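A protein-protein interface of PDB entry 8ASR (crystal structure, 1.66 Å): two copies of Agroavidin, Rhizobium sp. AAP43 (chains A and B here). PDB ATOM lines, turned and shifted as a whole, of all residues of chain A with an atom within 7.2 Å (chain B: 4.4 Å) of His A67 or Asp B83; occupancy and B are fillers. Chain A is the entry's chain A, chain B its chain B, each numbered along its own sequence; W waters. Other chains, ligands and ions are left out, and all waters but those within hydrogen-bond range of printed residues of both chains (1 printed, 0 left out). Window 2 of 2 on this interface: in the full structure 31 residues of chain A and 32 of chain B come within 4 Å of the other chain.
Val B76 touches His A65 (N to CB, 3.6 Å).
Val B76 touches His A67.
Val B76 touches Thr A70.
Thr A70 touches Arg B85.
A ring nitrogen (ND1) of His A67 sits at hydrogen-bond distance from the side-chain carboxylate (OD2) of Asp A15.
The backbone NH of His A65 sits at hydrogen-bond distance from the backbone carbonyl oxygen of Ala A72.
OD2 of Asp B83 lies within salt-bridge range of NE of Arg B85 (3.8 Å).
SG of Cys B84 forms a disulfide with SG of Cys B55 (2.1 Å).
Of chain B, only Val B76, Ser B78 and Asp B83 come within 4 Å of His A67.
Of the printed residues of chain B, Thr A70 touches Val B76 (3.9 Å) and Arg B85 (3.7 Å).
Of the printed residues of chain A, Val B76 touches His A65, His A67 and Thr A70.
Of the printed residues of chain A, Ser B78 touches His A67.
Of chain A, only His A67 comes within 4 Å of Asp B83.
Of the printed residues of chain A, Arg B85 touches Thr A70.
The nearest printed residue of chain B that does not touch His A67 is Trp B77 (5.7 Å).
The nearest printed residue of chain A that does not touch Val B76 is Ala A66 (4.04 Å).
Water W1 bridges OG of Ser B78 (2.7 Å) and ND1 of His A67 (3.5 Å).
No position is printed for both chains.
Of the 6 pairs that touch across the chains among the printed residues, none has its exchanged pair printed and touching as well.
Of the 16 printed residues of chain A, 3 touch a printed residue of chain B.
Hydrophobic or aromatic side chains of chain A within 4 Å of the printed part of chain B: His A65 and His A67.
Hydrophobic or aromatic side chains of chain B that line the printed part of chain A: Val B76.
Among the printed residues, 6 pairs touch across the chains.
NE2 of His A67 sits close to OG of Ser B78 (3.2 Å).
A ring nitrogen (NE2) of His A67 sits at hydrogen-bond distance from the side-chain carboxylate (OD2) of Asp B83, 3.0 Å away.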
ATOM      1  N   ASP A  13     -16.796 -27.611 -32.088  1.00  0.00           N
ATOM      2  CA  ASP A  13     -17.186 -26.235 -31.681  1.00  0.00           C
ATOM      3  C   ASP A  13     -18.576 -25.900 -32.214  1.00  0.00           C
ATOM      4  O   ASP A  13     -19.070 -26.582 -33.134  1.00  0.00           O
ATOM      5  CB  ASP A  13     -16.123 -25.218 -32.140  1.00  0.00           C
ATOM      6  CG  ASP A  13     -15.776 -25.181 -33.628  1.00  0.00           C
ATOM      7  OD1 ASP A  13     -16.643 -25.434 -34.493  1.00  0.00           O
ATOM      8  OD2 ASP A  13     -14.618 -24.861 -33.922  1.00  0.00           O
ATOM      9  N   PHE A  14     -19.165 -24.817 -31.716  1.00  0.00           N
ATOM     10  CA  PHE A  14     -20.464 -24.349 -32.237  1.00  0.00           C
ATOM     11  C   PHE A  14     -20.323 -23.790 -33.658  1.00  0.00           C
ATOM     12  O   PHE A  14     -21.321 -23.825 -34.412  1.00  0.00           O
ATOM     13  CB  PHE A  14     -21.079 -23.345 -31.266  1.00  0.00           C
ATOM     14  CG  PHE A  14     -21.516 -23.954 -29.963  1.00  0.00           C
ATOM     15  CD1 PHE A  14     -22.571 -24.854 -29.916  1.00  0.00           C
ATOM     16  CD2 PHE A  14     -20.947 -23.557 -28.764  1.00  0.00           C
ATOM     17  CE1 PHE A  14     -22.991 -25.371 -28.708  1.00  0.00           C
ATOM     18  CE2 PHE A  14     -21.390 -24.064 -27.557  1.00  0.00           C
ATOM     19  CZ  PHE A  14     -22.410 -24.984 -27.532  1.00  0.00           C
ATOM     20  N   ASP A  15     -19.188 -23.179 -33.980  1.00  0.00           N
ATOM     21  CA  ASP A  15     -18.989 -22.475 -35.271  1.00  0.00           C
ATOM     22  C   ASP A  15     -19.273 -23.436 -36.420  1.00  0.00           C
ATOM     23  O   ASP A  15     -19.967 -23.012 -37.387  1.00  0.00           O
ATOM     24  CB  ASP A  15     -17.582 -21.893 -35.421  1.00  0.00           C
ATOM     25  CG  ASP A  15     -17.158 -21.121 -34.193  1.00  0.00           C
ATOM     26  OD1 ASP A  15     -16.954 -21.771 -33.167  1.00  0.00           O
ATOM     27  OD2 ASP A  15     -17.120 -19.877 -34.283  1.00  0.00           O
ATOM     28  N   VAL A  36     -27.197 -21.720 -36.980  1.00  0.00           N
ATOM     29  CA  VAL A  36     -26.013 -20.862 -36.672  1.00  0.00           C
ATOM     30  C   VAL A  36     -25.514 -20.205 -37.969  1.00  0.00           C
ATOM     31  O   VAL A  36     -25.247 -20.961 -38.916  1.00  0.00           O
ATOM     32  CB  VAL A  36     -24.929 -21.712 -35.992  1.00  0.00           C
ATOM     33  CG1 VAL A  36     -23.733 -20.823 -35.651  1.00  0.00           C
ATOM     34  CG2 VAL A  36     -25.450 -22.475 -34.770  1.00  0.00           C
ATOM     35  N   LYS A  39     -21.072 -16.084 -38.824  1.00  0.00           N
ATOM     36  CA  LYS A  39     -20.413 -15.280 -37.757  1.00  0.00           C
ATOM     37  C   LYS A  39     -20.750 -15.807 -36.348  1.00  0.00           C
ATOM     38  O   LYS A  39     -20.251 -15.230 -35.373  1.00  0.00           O
ATOM     39  CB  LYS A  39     -20.827 -13.811 -37.867  1.00  0.00           C
ATOM     40  CG  LYS A  39     -19.996 -12.945 -38.790  1.00  0.00           C
ATOM     41  CD  LYS A  39     -20.236 -11.466 -38.553  1.00  0.00           C
ATOM     42  CE  LYS A  39     -19.432 -10.559 -39.466  1.00  0.00           C
ATOM     43  NZ  LYS A  39     -20.012  -9.192 -39.535  1.00  0.00           N
ATOM     44  N   GLY A  40     -21.511 -16.896 -36.225  1.00  0.00           N
ATOM     45  CA  GLY A  40     -21.909 -17.481 -34.921  1.00  0.00           C
ATOM     46  C   GLY A  40     -23.195 -16.867 -34.398  1.00  0.00           C
ATOM     47  O   GLY A  40     -23.572 -17.123 -33.242  1.00  0.00           O
ATOM     48  N   VAL A  42     -27.013 -16.877 -33.733  1.00  0.00           N
ATOM     49  CA  VAL A  42     -27.899 -18.055 -33.512  1.00  0.00           C
ATOM     50  C   VAL A  42     -29.337 -17.580 -33.626  1.00  0.00           C
ATOM     51  O   VAL A  42     -29.708 -16.564 -33.051  1.00  0.00           O
ATOM     52  CB  VAL A  42     -27.631 -18.774 -32.177  1.00  0.00           C
ATOM     53  CG1 VAL A  42     -28.611 -19.927 -31.972  1.00  0.00           C
ATOM     54  CG2 VAL A  42     -26.202 -19.232 -32.045  1.00  0.00           C
ATOM     55  N   HIS A  65     -25.848 -16.059 -29.734  1.00  0.00           N
ATOM     56  CA  HIS A  65     -24.498 -16.040 -30.312  1.00  0.00           C
ATOM     57  C   HIS A  65     -23.746 -17.250 -29.788  1.00  0.00           C
ATOM     58  O   HIS A  65     -23.894 -17.590 -28.597  1.00  0.00           O
ATOM     59  CB  HIS A  65     -23.737 -14.716 -30.041  1.00  0.00           C
ATOM     60  CG  HIS A  65     -24.309 -13.548 -30.766  1.00  0.00           C
ATOM     61  ND1 HIS A  65     -23.944 -13.248 -32.065  1.00  0.00           N
ATOM     62  CD2 HIS A  65     -25.306 -12.702 -30.447  1.00  0.00           C
ATOM     63  CE1 HIS A  65     -24.676 -12.232 -32.503  1.00  0.00           C
ATOM     64  NE2 HIS A  65     -25.528 -11.896 -31.531  1.00  0.00           N
ATOM     65  N   ALA A  66     -22.886 -17.818 -30.606  1.00  0.00           N
ATOM     66  CA  ALA A  66     -22.037 -18.937 -30.162  1.00  0.00           C
ATOM     67  C   ALA A  66     -20.648 -18.847 -30.805  1.00  0.00           C
ATOM     68  O   ALA A  66     -20.517 -18.282 -31.910  1.00  0.00           O
ATOM     69  CB  ALA A  66     -22.719 -20.223 -30.527  1.00  0.00           C
ATOM     70  N   HIS A  67     -19.662 -19.413 -30.122  1.00  0.00           N
ATOM     71  CA  HIS A  67     -18.278 -19.534 -30.611  1.00  0.00           C
ATOM     72  C   HIS A  67     -17.548 -20.551 -29.764  1.00  0.00           C
ATOM     73  O   HIS A  67     -17.670 -20.474 -28.531  1.00  0.00           O
ATOM     74  CB  HIS A  67     -17.537 -18.191 -30.559  1.00  0.00           C
ATOM     75  CG  HIS A  67     -16.126 -18.286 -31.017  1.00  0.00           C
ATOM     76  ND1 HIS A  67     -15.802 -18.555 -32.336  1.00  0.00           N
ATOM     77  CD2 HIS A  67     -14.966 -18.163 -30.338  1.00  0.00           C
ATOM     78  CE1 HIS A  67     -14.475 -18.568 -32.456  1.00  0.00           C
ATOM     79  NE2 HIS A  67     -13.947 -18.344 -31.237  1.00  0.00           N
ATOM     80  N   GLY A  68     -16.718 -21.355 -30.421  1.00  0.00           N
ATOM     81  CA  GLY A  68     -15.915 -22.363 -29.713  1.00  0.00           C
ATOM     82  C   GLY A  68     -16.823 -23.216 -28.852  1.00  0.00           C
ATOM     83  O   GLY A  68     -17.753 -23.870 -29.377  1.00  0.00           O
ATOM     84  N   SER A  69     -16.593 -23.192 -27.556  1.00  0.00           N
ATOM     85  CA  SER A  69     -17.298 -24.071 -26.592  1.00  0.00           C
ATOM     86  C   SER A  69     -18.312 -23.312 -25.755  1.00  0.00           C
ATOM     87  O   SER A  69     -18.785 -23.913 -24.802  1.00  0.00           O
ATOM     88  CB  SER A  69     -16.327 -24.803 -25.708  1.00  0.00           C
ATOM     89  OG  SER A  69     -15.645 -25.795 -26.468  1.00  0.00           O
ATOM     90  N   THR A  70     -18.674 -22.065 -26.120  1.00  0.00           N
ATOM     91  CA  THR A  70     -19.703 -21.333 -25.343  1.00  0.00           C
ATOM     92  C   THR A  70     -20.779 -20.724 -26.236  1.00  0.00           C
ATOM     93  O   THR A  70     -20.548 -20.470 -27.417  1.00  0.00           O
ATOM     94  CB  THR A  70     -19.142 -20.268 -24.399  1.00  0.00           C
ATOM     95  OG1 THR A  70     -18.697 -19.112 -25.117  1.00  0.00           O
ATOM     96  CG2 THR A  70     -18.031 -20.796 -23.516  1.00  0.00           C
ATOM     97  N   ILE A  71     -21.934 -20.522 -25.625  1.00  0.00           N
ATOM     98  CA  ILE A  71     -23.180 -20.075 -26.330  1.00  0.00           C
ATOM     99  C   ILE A  71     -24.008 -19.248 -25.348  1.00  0.00           C
ATOM    100  O   ILE A  71     -24.001 -19.536 -24.135  1.00  0.00           O
ATOM    101  CB  ILE A  71     -23.955 -21.264 -26.952  1.00  0.00           C
ATOM    102  CG1 ILE A  71     -25.162 -20.801 -27.771  1.00  0.00           C
ATOM    103  CG2 ILE A  71     -24.378 -22.264 -25.879  1.00  0.00           C
ATOM    104  CD1 ILE A  71     -25.790 -21.864 -28.674  1.00  0.00           C
ATOM    105  N   ALA A  72     -24.703 -18.225 -25.856  1.00  0.00           N
ATOM    106  CA  ALA A  72     -25.654 -17.425 -25.054  1.00  0.00           C
ATOM    107  C   ALA A  72     -26.869 -17.227 -25.931  1.00  0.00           C
ATOM    108  O   ALA A  72     -26.660 -17.019 -27.139  1.00  0.00           O
ATOM    109  CB  ALA A  72     -25.071 -16.096 -24.609  1.00  0.00           C
ATOM    110  N   GLY A  92     -24.090 -20.936 -21.603  1.00  0.00           N
ATOM    111  CA  GLY A  92     -23.579 -22.268 -21.272  1.00  0.00           C
ATOM    112  C   GLY A  92     -22.340 -22.652 -22.036  1.00  0.00           C
ATOM    113  O   GLY A  92     -21.893 -21.925 -22.944  1.00  0.00           O
ATOM    114  N   CYS B  55     -11.255  -8.711 -23.222  1.00  0.00           N
ATOM    115  CA  CYS B  55     -12.134  -8.296 -24.363  1.00  0.00           C
ATOM    116  C   CYS B  55     -12.723  -6.905 -24.066  1.00  0.00           C
ATOM    117  O   CYS B  55     -13.961  -6.729 -24.153  1.00  0.00           O
ATOM    118  CB  CYS B  55     -13.199  -9.365 -24.579  1.00  0.00           C
ATOM    119  SG  CYS B  55     -12.509 -10.902 -25.268  1.00  0.00           S
ATOM    120  N   VAL B  76     -21.603 -13.249 -27.477  1.00  0.00           N
ATOM    121  CA  VAL B  76     -20.416 -14.120 -27.325  1.00  0.00           C
ATOM    122  C   VAL B  76     -19.156 -13.252 -27.405  1.00  0.00           C
ATOM    123  O   VAL B  76     -19.086 -12.359 -28.252  1.00  0.00           O
ATOM    124  CB  VAL B  76     -20.431 -15.296 -28.318  1.00  0.00           C
ATOM    125  CG1 VAL B  76     -20.088 -14.886 -29.745  1.00  0.00           C
ATOM    126  CG2 VAL B  76     -19.505 -16.384 -27.811  1.00  0.00           C
ATOM    127  N   TRP B  77     -18.167 -13.517 -26.545  1.00  0.00           N
ATOM    128  CA  TRP B  77     -16.953 -12.670 -26.444  1.00  0.00           C
ATOM    129  C   TRP B  77     -15.915 -13.151 -27.442  1.00  0.00           C
ATOM    130  O   TRP B  77     -14.826 -13.565 -27.024  1.00  0.00           O
ATOM    131  CB  TRP B  77     -16.436 -12.645 -25.004  1.00  0.00           C
ATOM    132  CG  TRP B  77     -17.474 -12.124 -24.072  1.00  0.00           C
ATOM    133  CD1 TRP B  77     -18.304 -12.843 -23.263  1.00  0.00           C
ATOM    134  CD2 TRP B  77     -17.897 -10.760 -23.972  1.00  0.00           C
ATOM    135  NE1 TRP B  77     -19.154 -12.000 -22.595  1.00  0.00           N
ATOM    136  CE2 TRP B  77     -18.940 -10.717 -23.020  1.00  0.00           C
ATOM    137  CE3 TRP B  77     -17.415  -9.557 -24.504  1.00  0.00           C
ATOM    138  CZ2 TRP B  77     -19.543  -9.524 -22.646  1.00  0.00           C
ATOM    139  CZ3 TRP B  77     -18.017  -8.374 -24.126  1.00  0.00           C
ATOM    140  CH2 TRP B  77     -19.061  -8.364 -23.201  1.00  0.00           C
ATOM    141  N   SER B  78     -16.304 -13.162 -28.708  1.00  0.00           N
ATOM    142  CA  SER B  78     -15.429 -13.460 -29.881  1.00  0.00           C
ATOM    143  C   SER B  78     -15.911 -12.620 -31.065  1.00  0.00           C
ATOM    144  O   SER B  78     -17.147 -12.641 -31.338  1.00  0.00           O
ATOM    145  CB  SER B  78     -15.456 -14.935 -30.216  1.00  0.00           C
ATOM    146  OG  SER B  78     -14.615 -15.175 -31.349  1.00  0.00           O
ATOM    147  N   ALA B  82     -10.598 -10.398 -30.703  1.00  0.00           N
ATOM    148  CA  ALA B  82     -10.229 -10.888 -29.373  1.00  0.00           C
ATOM    149  C   ALA B  82     -11.314 -11.846 -28.919  1.00  0.00           C
ATOM    150  O   ALA B  82     -12.524 -11.487 -29.069  1.00  0.00           O
ATOM    151  CB  ALA B  82     -10.052  -9.744 -28.426  1.00  0.00           C
ATOM    152  N   ASP B  83     -10.886 -13.013 -28.441  1.00  0.00           N
ATOM    153  CA  ASP B  83     -11.749 -14.133 -28.037  1.00  0.00           C
ATOM    154  C   ASP B  83     -11.481 -14.377 -26.551  1.00  0.00           C
ATOM    155  O   ASP B  83     -10.308 -14.733 -26.215  1.00  0.00           O
ATOM    156  CB  ASP B  83     -11.511 -15.367 -28.929  1.00  0.00           C
ATOM    157  CG  ASP B  83     -12.259 -16.639 -28.503  1.00  0.00           C
ATOM    158  OD1 ASP B  83     -13.151 -16.543 -27.652  1.00  0.00           O
ATOM    159  OD2 ASP B  83     -11.956 -17.724 -29.045  1.00  0.00           O
ATOM    160  N   CYS B  84     -12.479 -14.176 -25.681  1.00  0.00           N
ATOM    161  CA  CYS B  84     -12.349 -14.501 -24.246  1.00  0.00           C
ATOM    162  C   CYS B  84     -12.981 -15.849 -23.878  1.00  0.00           C
ATOM    163  O   CYS B  84     -13.104 -16.118 -22.680  1.00  0.00           O
ATOM    164  CB  CYS B  84     -12.859 -13.351 -23.389  1.00  0.00           C
ATOM    165  SG  CYS B  84     -11.774 -11.925 -23.559  1.00  0.00           S
ATOM    166  N   ARG B  85     -13.267 -16.716 -24.852  1.00  0.00           N
ATOM    167  CA  ARG B  85     -13.734 -18.094 -24.557  1.00  0.00           C
ATOM    168  C   ARG B  85     -14.917 -18.027 -23.581  1.00  0.00           C
ATOM    169  O   ARG B  85     -14.993 -18.846 -22.641  1.00  0.00           O
ATOM    170  CB  ARG B  85     -12.599 -18.921 -23.936  1.00  0.00           C
ATOM    171  CG  ARG B  85     -11.514 -19.340 -24.915  1.00  0.00           C
ATOM    172  CD  ARG B  85     -10.633 -18.249 -25.468  1.00  0.00           C
ATOM    173  NE  ARG B  85      -9.561 -18.840 -26.285  1.00  0.00           N
ATOM    174  CZ  ARG B  85      -8.512 -18.187 -26.775  1.00  0.00           C
ATOM    175  NH1 ARG B  85      -7.634 -18.851 -27.508  1.00  0.00           N
ATOM    176  NH2 ARG B  85      -8.342 -16.885 -26.555  1.00  0.00           N
HETATM  177  O   HOH W   1     -16.291 -15.318 -33.508  1.00  0.00           O
